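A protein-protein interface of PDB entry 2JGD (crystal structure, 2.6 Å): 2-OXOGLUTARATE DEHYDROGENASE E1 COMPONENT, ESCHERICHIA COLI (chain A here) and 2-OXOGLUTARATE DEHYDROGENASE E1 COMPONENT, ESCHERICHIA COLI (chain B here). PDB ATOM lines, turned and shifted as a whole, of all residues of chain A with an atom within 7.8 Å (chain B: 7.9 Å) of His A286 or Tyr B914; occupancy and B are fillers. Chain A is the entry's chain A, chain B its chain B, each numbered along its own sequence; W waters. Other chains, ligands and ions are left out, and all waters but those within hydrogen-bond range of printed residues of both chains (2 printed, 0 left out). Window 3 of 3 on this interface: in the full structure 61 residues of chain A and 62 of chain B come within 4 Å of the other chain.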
ATOM      1  N   ASP A 277      -5.088 -21.118 -25.191  1.00  0.00           N
ATOM      2  CA  ASP A 277      -6.405 -21.614 -25.604  1.00  0.00           C
ATOM      3  C   ASP A 277      -7.046 -22.516 -24.553  1.00  0.00           C
ATOM      4  O   ASP A 277      -8.236 -22.404 -24.273  1.00  0.00           O
ATOM      5  CB  ASP A 277      -6.331 -22.316 -26.957  1.00  0.00           C
ATOM      6  CG  ASP A 277      -5.933 -21.379 -28.062  1.00  0.00           C
ATOM      7  OD1 ASP A 277      -6.141 -20.163 -27.903  1.00  0.00           O
ATOM      8  OD2 ASP A 277      -5.395 -21.852 -29.079  1.00  0.00           O
ATOM      9  N   ASP A 280      -8.050 -20.511 -21.453  1.00  0.00           N
ATOM     10  CA  ASP A 280      -9.277 -19.819 -21.827  1.00  0.00           C
ATOM     11  C   ASP A 280     -10.487 -20.700 -21.676  1.00  0.00           C
ATOM     12  O   ASP A 280     -11.513 -20.267 -21.172  1.00  0.00           O
ATOM     13  CB  ASP A 280      -9.198 -19.330 -23.267  1.00  0.00           C
ATOM     14  CG  ASP A 280      -8.339 -18.106 -23.409  1.00  0.00           C
ATOM     15  OD1 ASP A 280      -7.899 -17.600 -22.362  1.00  0.00           O
ATOM     16  OD2 ASP A 280      -8.099 -17.661 -24.552  1.00  0.00           O
ATOM     17  N   GLU A 281     -10.377 -21.936 -22.140  1.00  0.00           N
ATOM     18  CA  GLU A 281     -11.471 -22.864 -21.996  1.00  0.00           C
ATOM     19  C   GLU A 281     -11.908 -22.958 -20.534  1.00  0.00           C
ATOM     20  O   GLU A 281     -13.103 -22.954 -20.241  1.00  0.00           O
ATOM     21  CB  GLU A 281     -11.109 -24.241 -22.565  1.00  0.00           C
ATOM     22  CG  GLU A 281     -11.183 -24.329 -24.092  1.00  0.00           C
ATOM     23  CD  GLU A 281     -10.538 -25.603 -24.674  1.00  0.00           C
ATOM     24  OE1 GLU A 281     -10.518 -25.749 -25.921  1.00  0.00           O
ATOM     25  OE2 GLU A 281     -10.059 -26.454 -23.895  1.00  0.00           O
ATOM     26  N   PHE A 282     -10.944 -23.017 -19.618  1.00  0.00           N
ATOM     27  CA  PHE A 282     -11.251 -23.140 -18.178  1.00  0.00           C
ATOM     28  C   PHE A 282     -11.964 -21.919 -17.608  1.00  0.00           C
ATOM     29  O   PHE A 282     -12.647 -22.012 -16.592  1.00  0.00           O
ATOM     30  CB  PHE A 282      -9.981 -23.372 -17.375  1.00  0.00           C
ATOM     31  CG  PHE A 282      -9.590 -24.805 -17.259  1.00  0.00           C
ATOM     32  CD1 PHE A 282      -8.640 -25.350 -18.112  1.00  0.00           C
ATOM     33  CD2 PHE A 282     -10.140 -25.607 -16.279  1.00  0.00           C
ATOM     34  CE1 PHE A 282      -8.265 -26.679 -18.001  1.00  0.00           C
ATOM     35  CE2 PHE A 282      -9.761 -26.941 -16.161  1.00  0.00           C
ATOM     36  CZ  PHE A 282      -8.819 -27.473 -17.014  1.00  0.00           C
ATOM     37  N   ALA A 283     -11.767 -20.777 -18.253  1.00  0.00           N
ATOM     38  CA  ALA A 283     -12.361 -19.518 -17.819  1.00  0.00           C
ATOM     39  C   ALA A 283     -13.697 -19.277 -18.523  1.00  0.00           C
ATOM     40  O   ALA A 283     -14.372 -18.286 -18.266  1.00  0.00           O
ATOM     41  CB  ALA A 283     -11.404 -18.370 -18.111  1.00  0.00           C
ATOM     42  N   GLY A 284     -14.054 -20.174 -19.436  1.00  0.00           N
ATOM     43  CA  GLY A 284     -15.299 -20.060 -20.189  1.00  0.00           C
ATOM     44  C   GLY A 284     -15.232 -19.121 -21.381  1.00  0.00           C
ATOM     45  O   GLY A 284     -16.258 -18.593 -21.815  1.00  0.00           O
ATOM     46  N   LYS A 285     -14.032 -18.908 -21.917  1.00  0.00           N
ATOM     47  CA  LYS A 285     -13.873 -18.123 -23.147  1.00  0.00           C
ATOM     48  C   LYS A 285     -13.712 -19.026 -24.368  1.00  0.00           C
ATOM     49  O   LYS A 285     -12.872 -19.930 -24.376  1.00  0.00           O
ATOM     50  CB  LYS A 285     -12.685 -17.155 -23.044  1.00  0.00           C
ATOM     51  CG  LYS A 285     -12.437 -16.585 -21.643  1.00  0.00           C
ATOM     52  CD  LYS A 285     -13.478 -15.526 -21.246  1.00  0.00           C
ATOM     53  CE  LYS A 285     -13.121 -14.147 -21.790  1.00  0.00           C
ATOM     54  NZ  LYS A 285     -11.706 -14.098 -22.243  1.00  0.00           N
ATOM     55  N   HIS A 286     -14.532 -18.782 -25.392  1.00  0.00           N
ATOM     56  CA  HIS A 286     -14.507 -19.582 -26.619  1.00  0.00           C
ATOM     57  C   HIS A 286     -14.464 -18.675 -27.852  1.00  0.00           C
ATOM     58  O   HIS A 286     -14.603 -19.138 -28.986  1.00  0.00           O
ATOM     59  CB  HIS A 286     -15.728 -20.524 -26.690  1.00  0.00           C
ATOM     60  CG  HIS A 286     -15.952 -21.335 -25.442  1.00  0.00           C
ATOM     61  ND1 HIS A 286     -15.194 -22.447 -25.126  1.00  0.00           N
ATOM     62  CD2 HIS A 286     -16.866 -21.209 -24.446  1.00  0.00           C
ATOM     63  CE1 HIS A 286     -15.617 -22.957 -23.979  1.00  0.00           C
ATOM     64  NE2 HIS A 286     -16.631 -22.226 -23.547  1.00  0.00           N
ATOM     65  N   HIS A 289     -16.437 -21.424 -30.535  1.00  0.00           N
ATOM     66  CA  HIS A 289     -17.257 -22.305 -31.363  1.00  0.00           C
ATOM     67  C   HIS A 289     -18.596 -21.643 -31.692  1.00  0.00           C
ATOM     68  O   HIS A 289     -19.005 -20.682 -31.035  1.00  0.00           O
ATOM     69  CB  HIS A 289     -17.481 -23.650 -30.659  1.00  0.00           C
ATOM     70  N   LEU A 290     -19.268 -22.149 -32.718  1.00  0.00           N
ATOM     71  CA  LEU A 290     -20.622 -21.713 -33.018  1.00  0.00           C
ATOM     72  C   LEU A 290     -21.563 -22.883 -33.375  1.00  0.00           C
ATOM     73  O   LEU A 290     -22.471 -22.726 -34.192  1.00  0.00           O
ATOM     74  CB  LEU A 290     -20.609 -20.651 -34.122  1.00  0.00           C
ATOM     75  N   GLY A 291     -21.323 -24.053 -32.772  1.00  0.00           N
ATOM     76  CA  GLY A 291     -22.403 -24.981 -32.385  1.00  0.00           C
ATOM     77  C   GLY A 291     -22.545 -25.037 -30.870  1.00  0.00           C
ATOM     78  O   GLY A 291     -22.106 -24.129 -30.177  1.00  0.00           O
ATOM     79  N   THR A 292     -23.141 -26.100 -30.344  1.00  0.00           N
ATOM     80  CA  THR A 292     -23.459 -26.159 -28.911  1.00  0.00           C
ATOM     81  C   THR A 292     -22.330 -26.732 -28.048  1.00  0.00           C
ATOM     82  O   THR A 292     -22.347 -26.604 -26.836  1.00  0.00           O
ATOM     83  CB  THR A 292     -24.696 -26.987 -28.655  1.00  0.00           C
ATOM     84  OG1 THR A 292     -24.496 -28.307 -29.190  1.00  0.00           O
ATOM     85  CG2 THR A 292     -25.881 -26.347 -29.305  1.00  0.00           C
ATOM     86  N   GLY A 293     -21.370 -27.395 -28.668  1.00  0.00           N
ATOM     87  CA  GLY A 293     -20.121 -27.678 -27.983  1.00  0.00           C
ATOM     88  C   GLY A 293     -20.102 -28.938 -27.143  1.00  0.00           C
ATOM     89  O   GLY A 293     -21.069 -29.693 -27.079  1.00  0.00           O
ATOM     90  N   ASP A 294     -18.978 -29.174 -26.497  1.00  0.00           N
ATOM     91  CA  ASP A 294     -18.855 -30.305 -25.599  1.00  0.00           C
ATOM     92  C   ASP A 294     -17.721 -29.985 -24.610  1.00  0.00           C
ATOM     93  O   ASP A 294     -17.161 -28.891 -24.633  1.00  0.00           O
ATOM     94  CB  ASP A 294     -18.575 -31.574 -26.422  1.00  0.00           C
ATOM     95  CG  ASP A 294     -18.692 -32.845 -25.609  1.00  0.00           C
ATOM     96  OD1 ASP A 294     -19.166 -32.783 -24.455  1.00  0.00           O
ATOM     97  OD2 ASP A 294     -18.300 -33.912 -26.129  1.00  0.00           O
ATOM     98  N   VAL A 295     -17.416 -30.904 -23.716  1.00  0.00           N
ATOM     99  CA  VAL A 295     -16.530 -30.588 -22.608  1.00  0.00           C
ATOM    100  C   VAL A 295     -15.088 -30.703 -23.095  1.00  0.00           C
ATOM    101  O   VAL A 295     -14.826 -31.316 -24.136  1.00  0.00           O
ATOM    102  CB  VAL A 295     -16.792 -31.545 -21.390  1.00  0.00           C
ATOM    103  CG1 VAL A 295     -18.212 -31.345 -20.863  1.00  0.00           C
ATOM    104  CG2 VAL A 295     -16.633 -32.996 -21.801  1.00  0.00           C
ATOM    105  N   LYS A 296     -14.153 -30.119 -22.356  1.00  0.00           N
ATOM    106  CA  LYS A 296     -12.795 -29.924 -22.866  1.00  0.00           C
ATOM    107  C   LYS A 296     -12.047 -31.236 -23.037  1.00  0.00           C
ATOM    108  O   LYS A 296     -11.164 -31.330 -23.863  1.00  0.00           O
ATOM    109  CB  LYS A 296     -12.001 -28.964 -21.971  1.00  0.00           C
ATOM    110  CG  LYS A 296     -11.689 -29.520 -20.581  1.00  0.00           C
ATOM    111  CD  LYS A 296     -10.932 -28.484 -19.761  1.00  0.00           C
ATOM    112  CE  LYS A 296     -11.830 -27.338 -19.398  1.00  0.00           C
ATOM    113  NZ  LYS A 296     -12.881 -27.800 -18.444  1.00  0.00           N
ATOM    114  N   MET A 299     -12.025 -33.105 -26.568  1.00  0.00           N
ATOM    115  CA  MET A 299     -11.583 -32.309 -27.707  1.00  0.00           C
ATOM    116  C   MET A 299     -10.561 -33.040 -28.547  1.00  0.00           C
ATOM    117  O   MET A 299      -9.599 -33.611 -28.023  1.00  0.00           O
ATOM    118  CB  MET A 299     -11.067 -30.939 -27.287  1.00  0.00           C
ATOM    119  CG  MET A 299     -12.153 -30.016 -26.706  1.00  0.00           C
ATOM    120  SD  MET A 299     -13.569 -29.762 -27.820  1.00  0.00           S
ATOM    121  CE  MET A 299     -12.913 -28.491 -28.916  1.00  0.00           C
ATOM    122  N   GLN A 706     -22.791 -30.648 -33.867  1.00  0.00           N
ATOM    123  CA  GLN A 706     -23.121 -29.570 -32.946  1.00  0.00           C
ATOM    124  C   GLN A 706     -22.153 -29.609 -31.804  1.00  0.00           C
ATOM    125  O   GLN A 706     -21.727 -28.565 -31.283  1.00  0.00           O
ATOM    126  CB  GLN A 706     -24.534 -29.716 -32.408  1.00  0.00           C
ATOM    127  CG  GLN A 706     -25.604 -29.270 -33.372  1.00  0.00           C
ATOM    128  CD  GLN A 706     -25.532 -27.798 -33.666  1.00  0.00           C
ATOM    129  OE1 GLN A 706     -25.402 -26.969 -32.759  1.00  0.00           O
ATOM    130  NE2 GLN A 706     -25.654 -27.456 -34.927  1.00  0.00           N
ATOM    131  N   LYS A 707     -21.809 -30.827 -31.410  1.00  0.00           N
ATOM    132  CA  LYS A 707     -20.869 -31.035 -30.330  1.00  0.00           C
ATOM    133  C   LYS A 707     -19.461 -30.608 -30.765  1.00  0.00           C
ATOM    134  O   LYS A 707     -18.762 -29.951 -30.012  1.00  0.00           O
ATOM    135  CB  LYS A 707     -20.884 -32.508 -29.884  1.00  0.00           C
ATOM    136  CG  LYS A 707     -21.878 -32.803 -28.773  1.00  0.00           C
ATOM    137  CD  LYS A 707     -22.469 -34.172 -28.904  1.00  0.00           C
ATOM    138  CE  LYS A 707     -21.408 -35.227 -29.001  1.00  0.00           C
ATOM    139  NZ  LYS A 707     -21.997 -36.556 -28.770  1.00  0.00           N
ATOM    140  N   GLU B 723     -28.088 -30.126 -15.624  1.00  0.00           N
ATOM    141  CA  GLU B 723     -27.355 -29.409 -14.596  1.00  0.00           C
ATOM    142  C   GLU B 723     -26.085 -28.774 -15.184  1.00  0.00           C
ATOM    143  O   GLU B 723     -25.262 -28.227 -14.462  1.00  0.00           O
ATOM    144  CB  GLU B 723     -26.997 -30.354 -13.429  1.00  0.00           C
ATOM    145  CG  GLU B 723     -28.224 -30.909 -12.731  1.00  0.00           C
ATOM    146  CD  GLU B 723     -27.910 -32.108 -11.907  1.00  0.00           C
ATOM    147  OE1 GLU B 723     -26.758 -32.569 -11.987  1.00  0.00           O
ATOM    148  OE2 GLU B 723     -28.803 -32.593 -11.190  1.00  0.00           O
ATOM    149  N   GLY B 724     -25.936 -28.841 -16.496  1.00  0.00           N
ATOM    150  CA  GLY B 724     -24.851 -28.141 -17.138  1.00  0.00           C
ATOM    151  C   GLY B 724     -23.581 -28.964 -17.267  1.00  0.00           C
ATOM    152  O   GLY B 724     -22.528 -28.445 -17.602  1.00  0.00           O
ATOM    153  N   GLN B 725     -23.664 -30.257 -17.056  1.00  0.00           N
ATOM    154  CA  GLN B 725     -22.466 -31.060 -17.189  1.00  0.00           C
ATOM    155  C   GLN B 725     -22.302 -31.717 -18.547  1.00  0.00           C
ATOM    156  O   GLN B 725     -21.505 -32.627 -18.684  1.00  0.00           O
ATOM    157  CB  GLN B 725     -22.420 -32.112 -16.099  1.00  0.00           C
ATOM    158  CG  GLN B 725     -22.602 -31.545 -14.714  1.00  0.00           C
ATOM    159  CD  GLN B 725     -22.199 -32.527 -13.630  1.00  0.00           C
ATOM    160  OE1 GLN B 725     -22.756 -33.629 -13.527  1.00  0.00           O
ATOM    161  NE2 GLN B 725     -21.233 -32.132 -12.810  1.00  0.00           N
ATOM    162  N   GLY B 726     -23.037 -31.267 -19.561  1.00  0.00           N
ATOM    163  CA  GLY B 726     -22.723 -31.690 -20.945  1.00  0.00           C
ATOM    164  C   GLY B 726     -23.556 -32.841 -21.521  1.00  0.00           C
ATOM    165  O   GLY B 726     -24.355 -33.449 -20.817  1.00  0.00           O
ATOM    166  N   PRO B 727     -23.397 -33.111 -22.827  1.00  0.00           N
ATOM    167  CA  PRO B 727     -24.232 -34.043 -23.590  1.00  0.00           C
ATOM    168  C   PRO B 727     -24.361 -35.485 -23.050  1.00  0.00           C
ATOM    169  O   PRO B 727     -25.332 -36.169 -23.374  1.00  0.00           O
ATOM    170  CB  PRO B 727     -23.593 -34.033 -24.985  1.00  0.00           C
ATOM    171  CG  PRO B 727     -22.250 -33.405 -24.802  1.00  0.00           C
ATOM    172  CD  PRO B 727     -22.436 -32.422 -23.700  1.00  0.00           C
ATOM    173  N   ALA B 911     -27.462 -31.786 -24.761  1.00  0.00           N
ATOM    174  CA  ALA B 911     -27.161 -30.628 -23.913  1.00  0.00           C
ATOM    175  C   ALA B 911     -25.962 -29.880 -24.400  1.00  0.00           C
ATOM    176  O   ALA B 911     -25.092 -30.461 -25.048  1.00  0.00           O
ATOM    177  CB  ALA B 911     -26.957 -31.042 -22.485  1.00  0.00           C
ATOM    178  N   VAL B 912     -25.896 -28.592 -24.055  1.00  0.00           N
ATOM    179  CA  VAL B 912     -24.769 -27.751 -24.464  1.00  0.00           C
ATOM    180  C   VAL B 912     -23.472 -28.153 -23.744  1.00  0.00           C
ATOM    181  O   VAL B 912     -23.498 -28.764 -22.677  1.00  0.00           O
ATOM    182  CB  VAL B 912     -25.064 -26.276 -24.216  1.00  0.00           C
ATOM    183  CG1 VAL B 912     -26.325 -25.878 -24.935  1.00  0.00           C
ATOM    184  CG2 VAL B 912     -25.197 -25.997 -22.713  1.00  0.00           C
ATOM    185  N   GLY B 913     -22.341 -27.820 -24.339  1.00  0.00           N
ATOM    186  CA  GLY B 913     -21.061 -28.076 -23.713  1.00  0.00           C
ATOM    187  C   GLY B 913     -20.671 -27.108 -22.610  1.00  0.00           C
ATOM    188  O   GLY B 913     -19.820 -27.427 -21.802  1.00  0.00           O
ATOM    189  N   TYR B 914     -21.277 -25.923 -22.560  1.00  0.00           N
ATOM    190  CA  TYR B 914     -20.793 -24.890 -21.621  1.00  0.00           C
ATOM    191  C   TYR B 914     -21.781 -24.445 -20.521  1.00  0.00           C
ATOM    192  O   TYR B 914     -22.953 -24.163 -20.782  1.00  0.00           O
ATOM    193  CB  TYR B 914     -20.256 -23.677 -22.368  1.00  0.00           C
ATOM    194  CG  TYR B 914     -19.684 -23.951 -23.751  1.00  0.00           C
ATOM    195  CD1 TYR B 914     -20.295 -23.429 -24.884  1.00  0.00           C
ATOM    196  CD2 TYR B 914     -18.515 -24.683 -23.919  1.00  0.00           C
ATOM    197  CE1 TYR B 914     -19.768 -23.631 -26.153  1.00  0.00           C
ATOM    198  CE2 TYR B 914     -17.970 -24.892 -25.197  1.00  0.00           C
ATOM    199  CZ  TYR B 914     -18.607 -24.358 -26.307  1.00  0.00           C
ATOM    200  OH  TYR B 914     -18.098 -24.554 -27.583  1.00  0.00           O
ATOM    201  N   MET B 915     -21.279 -24.334 -19.299  1.00  0.00           N
ATOM    202  CA  MET B 915     -22.135 -24.138 -18.139  1.00  0.00           C
ATOM    203  C   MET B 915     -22.932 -22.837 -18.201  1.00  0.00           C
ATOM    204  O   MET B 915     -24.069 -22.772 -17.752  1.00  0.00           O
ATOM    205  CB  MET B 915     -21.312 -24.199 -16.843  1.00  0.00           C
ATOM    206  CG  MET B 915     -22.106 -23.843 -15.597  1.00  0.00           C
ATOM    207  SD  MET B 915     -23.094 -25.222 -14.994  1.00  0.00           S
ATOM    208  CE  MET B 915     -24.145 -24.421 -13.768  1.00  0.00           C
ATOM    209  N   SER B 916     -22.320 -21.791 -18.725  1.00  0.00           N
ATOM    210  CA  SER B 916     -22.931 -20.480 -18.661  1.00  0.00           C
ATOM    211  C   SER B 916     -24.162 -20.461 -19.555  1.00  0.00           C
ATOM    212  O   SER B 916     -25.245 -20.042 -19.142  1.00  0.00           O
ATOM    213  CB  SER B 916     -21.926 -19.393 -19.070  1.00  0.00           C
ATOM    214  OG  SER B 916     -21.529 -19.548 -20.425  1.00  0.00           O
ATOM    215  N   VAL B 917     -23.990 -20.952 -20.772  1.00  0.00           N
ATOM    216  CA  VAL B 917     -25.098 -21.165 -21.686  1.00  0.00           C
ATOM    217  C   VAL B 917     -26.218 -22.049 -21.081  1.00  0.00           C
ATOM    218  O   VAL B 917     -27.394 -21.685 -21.145  1.00  0.00           O
ATOM    219  CB  VAL B 917     -24.595 -21.750 -23.032  1.00  0.00           C
ATOM    220  CG1 VAL B 917     -25.751 -21.907 -24.024  1.00  0.00           C
ATOM    221  CG2 VAL B 917     -23.478 -20.844 -23.640  1.00  0.00           C
ATOM    222  N   HIS B 918     -25.862 -23.192 -20.485  1.00  0.00           N
ATOM    223  CA  HIS B 918     -26.841 -23.961 -19.708  1.00  0.00           C
ATOM    224  C   HIS B 918     -27.630 -23.046 -18.783  1.00  0.00           C
ATOM    225  O   HIS B 918     -28.863 -23.070 -18.745  1.00  0.00           O
ATOM    226  CB  HIS B 918     -26.179 -25.069 -18.878  1.00  0.00           C
ATOM    227  CG  HIS B 918     -27.113 -25.725 -17.898  1.00  0.00           C
ATOM    228  ND1 HIS B 918     -28.205 -26.471 -18.292  1.00  0.00           N
ATOM    229  CD2 HIS B 918     -27.158 -25.686 -16.545  1.00  0.00           C
ATOM    230  CE1 HIS B 918     -28.864 -26.885 -17.224  1.00  0.00           C
ATOM    231  NE2 HIS B 918     -28.247 -26.424 -16.152  1.00  0.00           N
ATOM    232  N   GLN B 919     -26.904 -22.223 -18.049  1.00  0.00           N
ATOM    233  CA  GLN B 919     -27.502 -21.450 -17.010  1.00  0.00           C
ATOM    234  C   GLN B 919     -28.525 -20.453 -17.552  1.00  0.00           C
ATOM    235  O   GLN B 919     -29.627 -20.365 -17.030  1.00  0.00           O
ATOM    236  CB  GLN B 919     -26.429 -20.807 -16.148  1.00  0.00           C
ATOM    237  CG  GLN B 919     -25.933 -21.735 -15.045  1.00  0.00           C
ATOM    238  CD  GLN B 919     -24.724 -21.198 -14.306  1.00  0.00           C
ATOM    239  OE1 GLN B 919     -24.438 -21.616 -13.178  1.00  0.00           O
ATOM    240  NE2 GLN B 919     -23.997 -20.271 -14.938  1.00  0.00           N
ATOM    241  N   LYS B 920     -28.202 -19.801 -18.665  1.00  0.00           N
ATOM    242  CA  LYS B 920     -29.123 -18.858 -19.286  1.00  0.00           C
ATOM    243  C   LYS B 920     -30.365 -19.589 -19.755  1.00  0.00           C
ATOM    244  O   LYS B 920     -31.497 -19.133 -19.536  1.00  0.00           O
ATOM    245  CB  LYS B 920     -28.469 -18.076 -20.449  1.00  0.00           C
ATOM    246  CG  LYS B 920     -29.353 -16.937 -20.985  1.00  0.00           C
ATOM    247  CD  LYS B 920     -28.677 -16.140 -22.106  1.00  0.00           C
ATOM    248  N   GLN B 921     -30.159 -20.745 -20.368  1.00  0.00           N
ATOM    249  CA  GLN B 921     -31.280 -21.534 -20.873  1.00  0.00           C
ATOM    250  C   GLN B 921     -32.232 -21.969 -19.760  1.00  0.00           C
ATOM    251  O   GLN B 921     -33.448 -21.828 -19.879  1.00  0.00           O
ATOM    252  CB  GLN B 921     -30.778 -22.744 -21.634  1.00  0.00           C
ATOM    253  CG  GLN B 921     -30.406 -22.442 -23.080  1.00  0.00           C
ATOM    254  CD  GLN B 921     -29.785 -23.626 -23.779  1.00  0.00           C
ATOM    255  OE1 GLN B 921     -29.334 -24.587 -23.138  1.00  0.00           O
ATOM    256  NE2 GLN B 921     -29.757 -23.571 -25.100  1.00  0.00           N
HETATM  257  O   HOH W   1     -23.672 -29.938 -27.211  1.00  0.00           O
HETATM  258  O   HOH W   2     -16.664 -27.055 -27.019  1.00  0.00           O
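The backbone carbonyl oxygen (O) of Thr A292 is in hydrogen-bond range of the backbone NH (N) of Gly B913, at 2.8 Å.
The backbone NH (N) of Gly A293 is in hydrogen-bond range of the backbone carbonyl oxygen (O) of Gln A706, 2.9 Å away.
The backbone NH (N) of Thr A292 is in hydrogen-bond range of the backbone carbonyl oxygen (O) of Gln A706, at 3.0 Å.
Among the printed residues, pairs that only touch across the chains: His A286 with Tyr B914 (3.1 Å), Asp A294 with Pro B727 (3.2 Å), His A289 with Tyr B914 (3.3 Å), Gly A293 with Gly B913 (3.6 Å), Thr A292 with Val B912 (3.6 Å), Asp A294 with Gly B913 (3.6 Å), Gly A293 with Tyr B914 (3.7 Å) and Thr A292 with Tyr B914 (3.99 Å).
His A286 touches one residue of chain B.
Printed residues of chain B within 4 Å of Gly A293: Gly B913 and Tyr B914.
Of the printed residues of chain B, Asp A294 touches Pro B727 and Gly B913.
Printed residues of chain A within 4 Å of Pro B727: Asp A294.
Of the printed residues of chain A, Val B912 touches Thr A292 (3.6 Å).
Printed residues of chain A within 4 Å of Tyr B914: His A286 (3.1 Å), His A289 (3.3 Å), Thr A292 (3.99 Å) and Gly A293 (3.7 Å).
Of the 19 printed residues of chain A, 5 touch a printed residue of chain B.
Hydrophobic or aromatic side chains of chain A that line the printed part of chain B: His A286 and His A289.
Along chain A the printed residues that touch a printed residue of chain B span positions 286 to 294.
Printed residues of chain B that touch a printed residue of chain A: Pro B727, Val B912, Gly B913 and Tyr B914.
Hydrophobic or aromatic side chains of chain B within 4 Å of the printed part of chain A: Pro B727, Val B912 and Tyr B914.
Among the printed residues, no Asp or Glu carboxylate lies within 4 Å of a Lys or Arg side-chain nitrogen of the other chain.
Water W1 lies within hydrogen-bond range of the backbone carbonyl oxygen (O) of Gly A293, the backbone carbonyl oxygen (O) of Ala B911 and the side-chain hydroxyl (OG1) of Thr A292.
Water W2 lies within hydrogen-bond range of OH of Tyr B914 (2.9 Å) and O of Asp A294 (3.1 Å).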
